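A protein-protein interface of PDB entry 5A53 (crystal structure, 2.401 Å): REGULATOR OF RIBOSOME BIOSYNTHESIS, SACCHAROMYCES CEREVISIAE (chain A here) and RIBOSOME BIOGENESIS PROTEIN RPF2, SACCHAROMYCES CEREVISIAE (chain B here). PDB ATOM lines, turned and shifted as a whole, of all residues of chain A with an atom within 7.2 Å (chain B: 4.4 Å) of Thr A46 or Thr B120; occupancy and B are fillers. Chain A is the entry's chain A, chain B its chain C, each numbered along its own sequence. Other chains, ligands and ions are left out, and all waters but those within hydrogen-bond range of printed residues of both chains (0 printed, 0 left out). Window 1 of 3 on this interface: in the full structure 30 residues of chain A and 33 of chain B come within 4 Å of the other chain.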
ATOM      1  N   LYS A   7     -18.179  17.839   4.094  1.00  0.00           N
ATOM      2  CA  LYS A   7     -19.522  17.788   4.653  1.00  0.00           C
ATOM      3  C   LYS A   7     -19.797  16.394   5.204  1.00  0.00           C
ATOM      4  O   LYS A   7     -19.335  15.404   4.636  1.00  0.00           O
ATOM      5  CB  LYS A   7     -20.564  18.156   3.593  1.00  0.00           C
ATOM      6  CG  LYS A   7     -20.713  19.650   3.341  1.00  0.00           C
ATOM      7  CD  LYS A   7     -21.381  19.911   1.998  1.00  0.00           C
ATOM      8  CE  LYS A   7     -21.661  21.391   1.786  1.00  0.00           C
ATOM      9  NZ  LYS A   7     -22.836  21.851   2.578  1.00  0.00           N
ATOM     10  N   LEU A  18     -27.733  20.693 -14.255  1.00  0.00           N
ATOM     11  CA  LEU A  18     -26.840  21.617 -13.555  1.00  0.00           C
ATOM     12  C   LEU A  18     -27.274  21.822 -12.105  1.00  0.00           C
ATOM     13  O   LEU A  18     -27.243  22.940 -11.589  1.00  0.00           O
ATOM     14  CB  LEU A  18     -26.782  22.966 -14.281  1.00  0.00           C
ATOM     15  CG  LEU A  18     -26.475  22.938 -15.781  1.00  0.00           C
ATOM     16  CD1 LEU A  18     -26.605  24.330 -16.379  1.00  0.00           C
ATOM     17  CD2 LEU A  18     -25.087  22.369 -16.040  1.00  0.00           C
ATOM     18  N   ALA A  19     -27.673  20.736 -11.449  1.00  0.00           N
ATOM     19  CA  ALA A  19     -28.242  20.827 -10.110  1.00  0.00           C
ATOM     20  C   ALA A  19     -27.460  20.024  -9.072  1.00  0.00           C
ATOM     21  O   ALA A  19     -26.890  18.977  -9.378  1.00  0.00           O
ATOM     22  CB  ALA A  19     -29.693  20.372 -10.134  1.00  0.00           C
ATOM     23  N   ALA A  20     -27.446  20.529  -7.843  1.00  0.00           N
ATOM     24  CA  ALA A  20     -26.840  19.826  -6.716  1.00  0.00           C
ATOM     25  C   ALA A  20     -27.830  19.745  -5.556  1.00  0.00           C
ATOM     26  O   ALA A  20     -28.603  20.675  -5.325  1.00  0.00           O
ATOM     27  CB  ALA A  20     -25.556  20.517  -6.281  1.00  0.00           C
ATOM     28  N   PHE A  21     -27.806  18.632  -4.830  1.00  0.00           N
ATOM     29  CA  PHE A  21     -28.743  18.425  -3.732  1.00  0.00           C
ATOM     30  C   PHE A  21     -28.018  18.139  -2.421  1.00  0.00           C
ATOM     31  O   PHE A  21     -27.243  17.187  -2.322  1.00  0.00           O
ATOM     32  CB  PHE A  21     -29.708  17.286  -4.066  1.00  0.00           C
ATOM     33  CG  PHE A  21     -30.320  17.399  -5.432  1.00  0.00           C
ATOM     34  CD1 PHE A  21     -31.191  18.434  -5.731  1.00  0.00           C
ATOM     35  CD2 PHE A  21     -30.024  16.473  -6.419  1.00  0.00           C
ATOM     36  CE1 PHE A  21     -31.751  18.546  -6.988  1.00  0.00           C
ATOM     37  CE2 PHE A  21     -30.584  16.577  -7.678  1.00  0.00           C
ATOM     38  CZ  PHE A  21     -31.450  17.614  -7.964  1.00  0.00           C
ATOM     39  N   ASP A  22     -28.279  18.972  -1.419  1.00  0.00           N
ATOM     40  CA  ASP A  22     -27.602  18.876  -0.131  1.00  0.00           C
ATOM     41  C   ASP A  22     -28.582  18.501   0.979  1.00  0.00           C
ATOM     42  O   ASP A  22     -29.519  19.245   1.270  1.00  0.00           O
ATOM     43  CB  ASP A  22     -26.904  20.202   0.192  1.00  0.00           C
ATOM     44  CG  ASP A  22     -26.189  20.182   1.530  1.00  0.00           C
ATOM     45  OD1 ASP A  22     -25.856  19.082   2.020  1.00  0.00           O
ATOM     46  OD2 ASP A  22     -25.954  21.273   2.090  1.00  0.00           O
ATOM     47  N   GLU A  40     -26.052  35.921   5.256  1.00  0.00           N
ATOM     48  CA  GLU A  40     -24.651  35.525   5.212  1.00  0.00           C
ATOM     49  C   GLU A  40     -24.559  34.005   5.226  1.00  0.00           C
ATOM     50  O   GLU A  40     -23.715  33.418   4.552  1.00  0.00           O
ATOM     51  CB  GLU A  40     -23.861  36.106   6.386  1.00  0.00           C
ATOM     52  CG  GLU A  40     -22.660  36.940   5.961  1.00  0.00           C
ATOM     53  CD  GLU A  40     -21.840  37.446   7.133  1.00  0.00           C
ATOM     54  OE1 GLU A  40     -21.795  36.755   8.173  1.00  0.00           O
ATOM     55  OE2 GLU A  40     -21.244  38.541   7.024  1.00  0.00           O
ATOM     56  N   LYS A  41     -25.444  33.377   5.993  1.00  0.00           N
ATOM     57  CA  LYS A  41     -25.467  31.924   6.109  1.00  0.00           C
ATOM     58  C   LYS A  41     -26.036  31.267   4.855  1.00  0.00           C
ATOM     59  O   LYS A  41     -25.537  30.233   4.414  1.00  0.00           O
ATOM     60  CB  LYS A  41     -26.275  31.497   7.336  1.00  0.00           C
ATOM     61  CG  LYS A  41     -25.697  31.982   8.654  1.00  0.00           C
ATOM     62  CD  LYS A  41     -24.310  31.406   8.887  1.00  0.00           C
ATOM     63  CE  LYS A  41     -23.692  31.945  10.166  1.00  0.00           C
ATOM     64  NZ  LYS A  41     -24.463  31.540  11.373  1.00  0.00           N
ATOM     65  N   ILE A  42     -27.082  31.866   4.291  1.00  0.00           N
ATOM     66  CA  ILE A  42     -27.682  31.356   3.062  1.00  0.00           C
ATOM     67  C   ILE A  42     -26.656  31.322   1.936  1.00  0.00           C
ATOM     68  O   ILE A  42     -26.493  30.305   1.262  1.00  0.00           O
ATOM     69  CB  ILE A  42     -28.882  32.211   2.604  1.00  0.00           C
ATOM     70  CG1 ILE A  42     -29.759  32.605   3.794  1.00  0.00           C
ATOM     71  CG2 ILE A  42     -29.686  31.475   1.535  1.00  0.00           C
ATOM     72  CD1 ILE A  42     -30.726  31.538   4.214  1.00  0.00           C
ATOM     73  N   LYS A  43     -25.967  32.442   1.744  1.00  0.00           N
ATOM     74  CA  LYS A  43     -24.993  32.573   0.667  1.00  0.00           C
ATOM     75  C   LYS A  43     -23.779  31.675   0.884  1.00  0.00           C
ATOM     76  O   LYS A  43     -23.314  31.017  -0.047  1.00  0.00           O
ATOM     77  CB  LYS A  43     -24.546  34.031   0.524  1.00  0.00           C
ATOM     78  CG  LYS A  43     -23.554  34.259  -0.604  1.00  0.00           C
ATOM     79  CD  LYS A  43     -23.419  35.733  -0.949  1.00  0.00           C
ATOM     80  CE  LYS A  43     -22.486  36.447   0.013  1.00  0.00           C
ATOM     81  NZ  LYS A  43     -22.175  37.825  -0.453  1.00  0.00           N
ATOM     82  N   SER A  44     -23.270  31.654   2.113  1.00  0.00           N
ATOM     83  CA  SER A  44     -22.094  30.853   2.448  1.00  0.00           C
ATOM     84  C   SER A  44     -22.348  29.372   2.203  1.00  0.00           C
ATOM     85  O   SER A  44     -21.508  28.674   1.634  1.00  0.00           O
ATOM     86  CB  SER A  44     -21.682  31.076   3.904  1.00  0.00           C
ATOM     87  OG  SER A  44     -20.877  30.010   4.373  1.00  0.00           O
ATOM     88  N   LEU A  45     -23.511  28.898   2.636  1.00  0.00           N
ATOM     89  CA  LEU A  45     -23.901  27.512   2.419  1.00  0.00           C
ATOM     90  C   LEU A  45     -24.097  27.230   0.932  1.00  0.00           C
ATOM     91  O   LEU A  45     -23.691  26.182   0.431  1.00  0.00           O
ATOM     92  CB  LEU A  45     -25.178  27.188   3.194  1.00  0.00           C
ATOM     93  CG  LEU A  45     -25.796  25.811   2.958  1.00  0.00           C
ATOM     94  CD1 LEU A  45     -24.809  24.707   3.307  1.00  0.00           C
ATOM     95  CD2 LEU A  45     -27.072  25.670   3.769  1.00  0.00           C
ATOM     96  N   THR A  46     -24.720  28.175   0.235  1.00  0.00           N
ATOM     97  CA  THR A  46     -24.931  28.055  -1.203  1.00  0.00           C
ATOM     98  C   THR A  46     -23.597  28.018  -1.941  1.00  0.00           C
ATOM     99  O   THR A  46     -23.419  27.242  -2.879  1.00  0.00           O
ATOM    100  CB  THR A  46     -25.782  29.218  -1.751  1.00  0.00           C
ATOM    101  OG1 THR A  46     -27.045  29.251  -1.076  1.00  0.00           O
ATOM    102  CG2 THR A  46     -26.019  29.052  -3.244  1.00  0.00           C
ATOM    103  N   ARG A  47     -22.662  28.855  -1.502  1.00  0.00           N
ATOM    104  CA  ARG A  47     -21.345  28.945  -2.126  1.00  0.00           C
ATOM    105  C   ARG A  47     -20.612  27.610  -2.077  1.00  0.00           C
ATOM    106  O   ARG A  47     -19.935  27.228  -3.033  1.00  0.00           O
ATOM    107  CB  ARG A  47     -20.505  30.027  -1.444  1.00  0.00           C
ATOM    108  CG  ARG A  47     -19.270  30.438  -2.226  1.00  0.00           C
ATOM    109  CD  ARG A  47     -18.046  30.515  -1.329  1.00  0.00           C
ATOM    110  NE  ARG A  47     -17.646  29.198  -0.840  1.00  0.00           N
ATOM    111  CZ  ARG A  47     -16.808  28.388  -1.479  1.00  0.00           C
ATOM    112  NH1 ARG A  47     -16.277  28.759  -2.636  1.00  0.00           N
ATOM    113  NH2 ARG A  47     -16.499  27.207  -0.961  1.00  0.00           N
ATOM    114  N   ASP A  48     -20.752  26.902  -0.960  1.00  0.00           N
ATOM    115  CA  ASP A  48     -20.123  25.599  -0.794  1.00  0.00           C
ATOM    116  C   ASP A  48     -20.674  24.586  -1.792  1.00  0.00           C
ATOM    117  O   ASP A  48     -19.923  23.811  -2.385  1.00  0.00           O
ATOM    118  CB  ASP A  48     -20.320  25.086   0.635  1.00  0.00           C
ATOM    119  CG  ASP A  48     -19.469  25.832   1.645  1.00  0.00           C
ATOM    120  OD1 ASP A  48     -18.554  26.571   1.225  1.00  0.00           O
ATOM    121  OD2 ASP A  48     -19.712  25.673   2.859  1.00  0.00           O
ATOM    122  N   ASN A  49     -21.991  24.600  -1.975  1.00  0.00           N
ATOM    123  CA  ASN A  49     -22.643  23.668  -2.886  1.00  0.00           C
ATOM    124  C   ASN A  49     -22.370  24.010  -4.348  1.00  0.00           C
ATOM    125  O   ASN A  49     -22.234  23.117  -5.184  1.00  0.00           O
ATOM    126  CB  ASN A  49     -24.148  23.636  -2.623  1.00  0.00           C
ATOM    127  CG  ASN A  49     -24.488  23.027  -1.278  1.00  0.00           C
ATOM    128  OD1 ASN A  49     -23.774  22.156  -0.781  1.00  0.00           O
ATOM    129  ND2 ASN A  49     -25.581  23.483  -0.680  1.00  0.00           N
ATOM    130  N   VAL A  50     -22.293  25.302  -4.650  1.00  0.00           N
ATOM    131  CA  VAL A  50     -21.943  25.750  -5.992  1.00  0.00           C
ATOM    132  C   VAL A  50     -20.512  25.332  -6.319  1.00  0.00           C
ATOM    133  O   VAL A  50     -20.224  24.869  -7.424  1.00  0.00           O
ATOM    134  CB  VAL A  50     -22.091  27.280  -6.140  1.00  0.00           C
ATOM    135  CG1 VAL A  50     -21.473  27.758  -7.444  1.00  0.00           C
ATOM    136  CG2 VAL A  50     -23.557  27.683  -6.062  1.00  0.00           C
ATOM    137  N   GLN A  51     -19.624  25.487  -5.342  1.00  0.00           N
ATOM    138  CA  GLN A  51     -18.233  25.071  -5.487  1.00  0.00           C
ATOM    139  C   GLN A  51     -18.147  23.584  -5.814  1.00  0.00           C
ATOM    140  O   GLN A  51     -17.462  23.184  -6.754  1.00  0.00           O
ATOM    141  CB  GLN A  51     -17.446  25.378  -4.212  1.00  0.00           C
ATOM    142  CG  GLN A  51     -15.970  25.016  -4.287  1.00  0.00           C
ATOM    143  CD  GLN A  51     -15.173  25.984  -5.138  1.00  0.00           C
ATOM    144  OE1 GLN A  51     -15.037  27.159  -4.799  1.00  0.00           O
ATOM    145  NE2 GLN A  51     -14.641  25.493  -6.252  1.00  0.00           N
ATOM    146  N   LEU A  52     -18.854  22.771  -5.033  1.00  0.00           N
ATOM    147  CA  LEU A  52     -18.895  21.330  -5.253  1.00  0.00           C
ATOM    148  C   LEU A  52     -19.520  20.994  -6.604  1.00  0.00           C
ATOM    149  O   LEU A  52     -19.090  20.061  -7.283  1.00  0.00           O
ATOM    150  CB  LEU A  52     -19.670  20.636  -4.131  1.00  0.00           C
ATOM    151  CG  LEU A  52     -19.012  20.604  -2.750  1.00  0.00           C
ATOM    152  CD1 LEU A  52     -20.018  20.178  -1.695  1.00  0.00           C
ATOM    153  CD2 LEU A  52     -17.808  19.672  -2.747  1.00  0.00           C
ATOM    154  N   LEU A  53     -20.537  21.760  -6.987  1.00  0.00           N
ATOM    155  CA  LEU A  53     -21.208  21.567  -8.267  1.00  0.00           C
ATOM    156  C   LEU A  53     -20.262  21.859  -9.428  1.00  0.00           C
ATOM    157  O   LEU A  53     -20.161  21.074 -10.370  1.00  0.00           O
ATOM    158  CB  LEU A  53     -22.451  22.453  -8.360  1.00  0.00           C
ATOM    159  CG  LEU A  53     -23.219  22.436  -9.684  1.00  0.00           C
ATOM    160  CD1 LEU A  53     -23.703  21.034 -10.008  1.00  0.00           C
ATOM    161  CD2 LEU A  53     -24.388  23.406  -9.638  1.00  0.00           C
ATOM    162  N   PHE B 119     -28.609  25.034 -10.213  1.00  0.00           N
ATOM    163  CA  PHE B 119     -29.499  24.821  -9.078  1.00  0.00           C
ATOM    164  C   PHE B 119     -28.756  24.251  -7.877  1.00  0.00           C
ATOM    165  O   PHE B 119     -27.893  23.387  -8.025  1.00  0.00           O
ATOM    166  CB  PHE B 119     -30.641  23.868  -9.446  1.00  0.00           C
ATOM    167  CG  PHE B 119     -31.606  24.421 -10.454  1.00  0.00           C
ATOM    168  CD1 PHE B 119     -31.405  24.221 -11.811  1.00  0.00           C
ATOM    169  CD2 PHE B 119     -32.733  25.114 -10.044  1.00  0.00           C
ATOM    170  CE1 PHE B 119     -32.301  24.717 -12.739  1.00  0.00           C
ATOM    171  CE2 PHE B 119     -33.633  25.612 -10.967  1.00  0.00           C
ATOM    172  CZ  PHE B 119     -33.417  25.412 -12.317  1.00  0.00           C
ATOM    173  N   THR B 120     -29.096  24.739  -6.688  1.00  0.00           N
ATOM    174  CA  THR B 120     -28.685  24.090  -5.447  1.00  0.00           C
ATOM    175  C   THR B 120     -29.874  24.033  -4.496  1.00  0.00           C
ATOM    176  O   THR B 120     -30.510  25.051  -4.222  1.00  0.00           O
ATOM    177  CB  THR B 120     -27.509  24.812  -4.752  1.00  0.00           C
ATOM    178  OG1 THR B 120     -27.885  26.157  -4.429  1.00  0.00           O
ATOM    179  CG2 THR B 120     -26.268  24.820  -5.636  1.00  0.00           C
ATOM    180  N   PHE B 121     -30.177  22.834  -4.009  1.00  0.00           N
ATOM    181  CA  PHE B 121     -31.261  22.647  -3.054  1.00  0.00           C
ATOM    182  C   PHE B 121     -30.708  22.230  -1.694  1.00  0.00           C
ATOM    183  O   PHE B 121     -30.036  21.206  -1.577  1.00  0.00           O
ATOM    184  CB  PHE B 121     -32.258  21.599  -3.561  1.00  0.00           C
ATOM    185  CG  PHE B 121     -33.047  22.039  -4.764  1.00  0.00           C
ATOM    186  CD1 PHE B 121     -32.520  21.912  -6.041  1.00  0.00           C
ATOM    187  CD2 PHE B 121     -34.318  22.571  -4.619  1.00  0.00           C
ATOM    188  CE1 PHE B 121     -33.245  22.312  -7.148  1.00  0.00           C
ATOM    189  CE2 PHE B 121     -35.047  22.976  -5.724  1.00  0.00           C
ATOM    190  CZ  PHE B 121     -34.510  22.845  -6.989  1.00  0.00           C
ATOM    191  N   GLN B 122     -30.989  23.031  -0.671  1.00  0.00           N
ATOM    192  CA  GLN B 122     -30.538  22.723   0.681  1.00  0.00           C
ATOM    193  C   GLN B 122     -31.694  22.255   1.557  1.00  0.00           C
ATOM    194  O   GLN B 122     -32.655  22.990   1.783  1.00  0.00           O
ATOM    195  CB  GLN B 122     -29.859  23.940   1.318  1.00  0.00           C
ATOM    196  CG  GLN B 122     -28.490  24.272   0.745  1.00  0.00           C
ATOM    197  CD  GLN B 122     -28.569  25.059  -0.548  1.00  0.00           C
ATOM    198  OE1 GLN B 122     -28.154  24.583  -1.603  1.00  0.00           O
ATOM    199  NE2 GLN B 122     -29.100  26.272  -0.471  1.00  0.00           N
ATOM    200  N   VAL B 159     -26.834  31.113 -10.229  1.00  0.00           N
ATOM    201  CA  VAL B 159     -27.389  29.946  -9.557  1.00  0.00           C
ATOM    202  C   VAL B 159     -28.715  30.287  -8.878  1.00  0.00           C
ATOM    203  O   VAL B 159     -28.872  31.362  -8.296  1.00  0.00           O
ATOM    204  CB  VAL B 159     -26.400  29.374  -8.510  1.00  0.00           C
ATOM    205  CG1 VAL B 159     -25.985  30.449  -7.514  1.00  0.00           C
ATOM    206  CG2 VAL B 159     -26.997  28.166  -7.794  1.00  0.00           C
ATOM    207  N   ILE B 160     -29.675  29.375  -8.981  1.00  0.00           N
ATOM    208  CA  ILE B 160     -30.914  29.486  -8.228  1.00  0.00           C
ATOM    209  C   ILE B 160     -30.820  28.600  -6.991  1.00  0.00           C
ATOM    210  O   ILE B 160     -30.691  27.381  -7.096  1.00  0.00           O
ATOM    211  CB  ILE B 160     -32.138  29.086  -9.072  1.00  0.00           C
ATOM    212  CG1 ILE B 160     -32.270  30.015 -10.281  1.00  0.00           C
ATOM    213  CG2 ILE B 160     -33.402  29.125  -8.230  1.00  0.00           C
ATOM    214  CD1 ILE B 160     -33.412  29.659 -11.208  1.00  0.00           C
ATOM    215  N   SER B 161     -30.871  29.224  -5.819  1.00  0.00           N
ATOM    216  CA  SER B 161     -30.716  28.502  -4.563  1.00  0.00           C
ATOM    217  C   SER B 161     -32.026  28.440  -3.787  1.00  0.00           C
ATOM    218  O   SER B 161     -32.695  29.456  -3.602  1.00  0.00           O
ATOM    219  CB  SER B 161     -29.631  29.156  -3.706  1.00  0.00           C
ATOM    220  OG  SER B 161     -29.549  28.549  -2.429  1.00  0.00           O
ATOM    221  N   MET B 162     -32.389  27.245  -3.335  1.00  0.00           N
ATOM    222  CA  MET B 162     -33.598  27.071  -2.538  1.00  0.00           C
ATOM    223  C   MET B 162     -33.294  26.319  -1.248  1.00  0.00           C
ATOM    224  O   MET B 162     -32.802  25.191  -1.271  1.00  0.00           O
ATOM    225  CB  MET B 162     -34.672  26.344  -3.346  1.00  0.00           C
ATOM    226  CG  MET B 162     -35.078  27.087  -4.607  1.00  0.00           C
ATOM    227  SD  MET B 162     -36.634  26.519  -5.305  1.00  0.00           S
ATOM    228  CE  MET B 162     -37.803  27.425  -4.299  1.00  0.00           C
ATOM    229  N   TYR B 182     -28.045  34.068  -7.061  1.00  0.00           N
ATOM    230  CA  TYR B 182     -26.692  34.613  -6.985  1.00  0.00           C
ATOM    231  C   TYR B 182     -25.984  34.588  -8.334  1.00  0.00           C
ATOM    232  O   TYR B 182     -26.189  33.677  -9.134  1.00  0.00           O
ATOM    233  CB  TYR B 182     -25.848  33.833  -5.973  1.00  0.00           C
ATOM    234  CG  TYR B 182     -26.424  33.758  -4.579  1.00  0.00           C
ATOM    235  CD1 TYR B 182     -26.198  34.770  -3.657  1.00  0.00           C
ATOM    236  CD2 TYR B 182     -27.174  32.662  -4.176  1.00  0.00           C
ATOM    237  CE1 TYR B 182     -26.715  34.702  -2.378  1.00  0.00           C
ATOM    238  CE2 TYR B 182     -27.695  32.583  -2.898  1.00  0.00           C
ATOM    239  CZ  TYR B 182     -27.462  33.606  -2.003  1.00  0.00           C
ATOM    240  OH  TYR B 182     -27.979  33.531  -0.731  1.00  0.00           O
ATOM    241  N   LEU B 201     -19.937  34.211  -4.477  1.00  0.00           N
ATOM    242  CA  LEU B 201     -21.273  34.558  -4.951  1.00  0.00           C
ATOM    243  C   LEU B 201     -21.677  35.987  -4.605  1.00  0.00           C
ATOM    244  O   LEU B 201     -21.292  36.521  -3.565  1.00  0.00           O
ATOM    245  CB  LEU B 201     -22.312  33.594  -4.377  1.00  0.00           C
ATOM    246  CG  LEU B 201     -22.140  32.099  -4.639  1.00  0.00           C
ATOM    247  CD1 LEU B 201     -23.284  31.334  -4.000  1.00  0.00           C
ATOM    248  CD2 LEU B 201     -22.064  31.813  -6.130  1.00  0.00           C
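N of Phe B121 lies within hydrogen-bond range of O of Ala A20 (3.0 Å). The backbone NH (N) of Lys A43 sits at hydrogen-bond distance from the side-chain hydroxyl (OH) of Tyr B182, 3.4 Å away. The backbone carbonyl oxygen of Leu A18 is in hydrogen-bond range of the backbone NH of Phe B119, 2.9 Å away. NZ of Lys A43 lies close to O of Leu B201, 3.5 Å away. OG1 of Thr A46 is in hydrogen-bond range of OG of Ser B161. The backbone NH (N) of Asp A22 sits at hydrogen-bond distance from the backbone carbonyl oxygen (O) of Phe B121 (2.8 Å). N of Ala A20 lies within hydrogen-bond range of O of Phe B119, at 2.9 Å. The side-chain amide nitrogen (ND2) of Asn A49 sits at hydrogen-bond distance from the side-chain amide oxygen (OE1) of Gln B122 (2.9 Å).
O of Leu A45 lies within hydrogen-bond range of ND2 of Asn A49 (3.5 Å). The backbone carbonyl oxygen (O) of Thr B120 lies within hydrogen-bond range of the backbone NH (N) of Met B162 (3.0 Å). The backbone carbonyl oxygen (O) of Ile A42 is in hydrogen-bond range of the side-chain hydroxyl (OG1) of Thr A46 (2.6 Å). The side-chain hydroxyl (OG1) of Thr B120 sits close to the side-chain amide oxygen (OE1) of Gln B122, at 3.2 Å. The side-chain carboxylate (OD2) of Asp A22 lies within salt-bridge range of the side-chain amino group (NZ) of Lys A7, at 3.2 Å. O of Ile B160 sits at hydrogen-bond distance from N of Thr B120 (3.1 Å).
CA of Thr B120 touches O of Ala A20, 3.4 Å away. Phe B121 touches Phe A21. O of Asp A22 touches CA of Gln B122, 3.7 Å away. Tyr B182 touches Ile A42 (OH to CG2, 3.5 Å). CD2 of Leu A45 touches CG of Gln B122, 3.6 Å away. Thr A46 touches Leu B201. Leu B201 touches Arg A47 (CD1 to N, 3.6 Å). Asn A49 touches Thr B120. Val A50 touches Thr B120. CG2 of Val B159 touches CG2 of Val A50 (3.9 Å).
Printed residues of chain B within 4 Å of Ile A42: Tyr B182. Gln A51 touches none of the printed residues of chain B. Thr B120 touches just these residues of chain A: Ala A20 (3.4 Å), Thr A46 (3.6 Å), Asn A49 (3.9 Å) and Val A50 (3.97 Å). Of the printed residues of chain A, Gln B122 touches Asp A22, Leu A45, Thr A46 and Asn A49. Ile B160 touches none of the printed residues of chain A. The nearest residue of chain A that does not touch Thr B120 is Leu A53 (4.6 Å).
Of the 20 printed residues of chain A, 13 touch a printed residue of chain B. Printed residues of chain A that touch a printed residue of chain B: Leu A18, Ala A19, Ala A20, Phe A21, Asp A22, Ile A42, Lys A43, Leu A45, Thr A46, Arg A47, Asn A49, Val A50 and Leu A53. Of the 10 printed residues of chain B, 8 touch a printed residue of chain A. Hydrophobic or aromatic side chains of chain B within 4 Å of the printed part of chain A: Phe B119, Phe B121, Val B159, Tyr B182 and Leu B201. Among the printed residues, no Asp or Glu carboxylate lies within 4 Å of a Lys or Arg side-chain nitrogen of the other chain.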
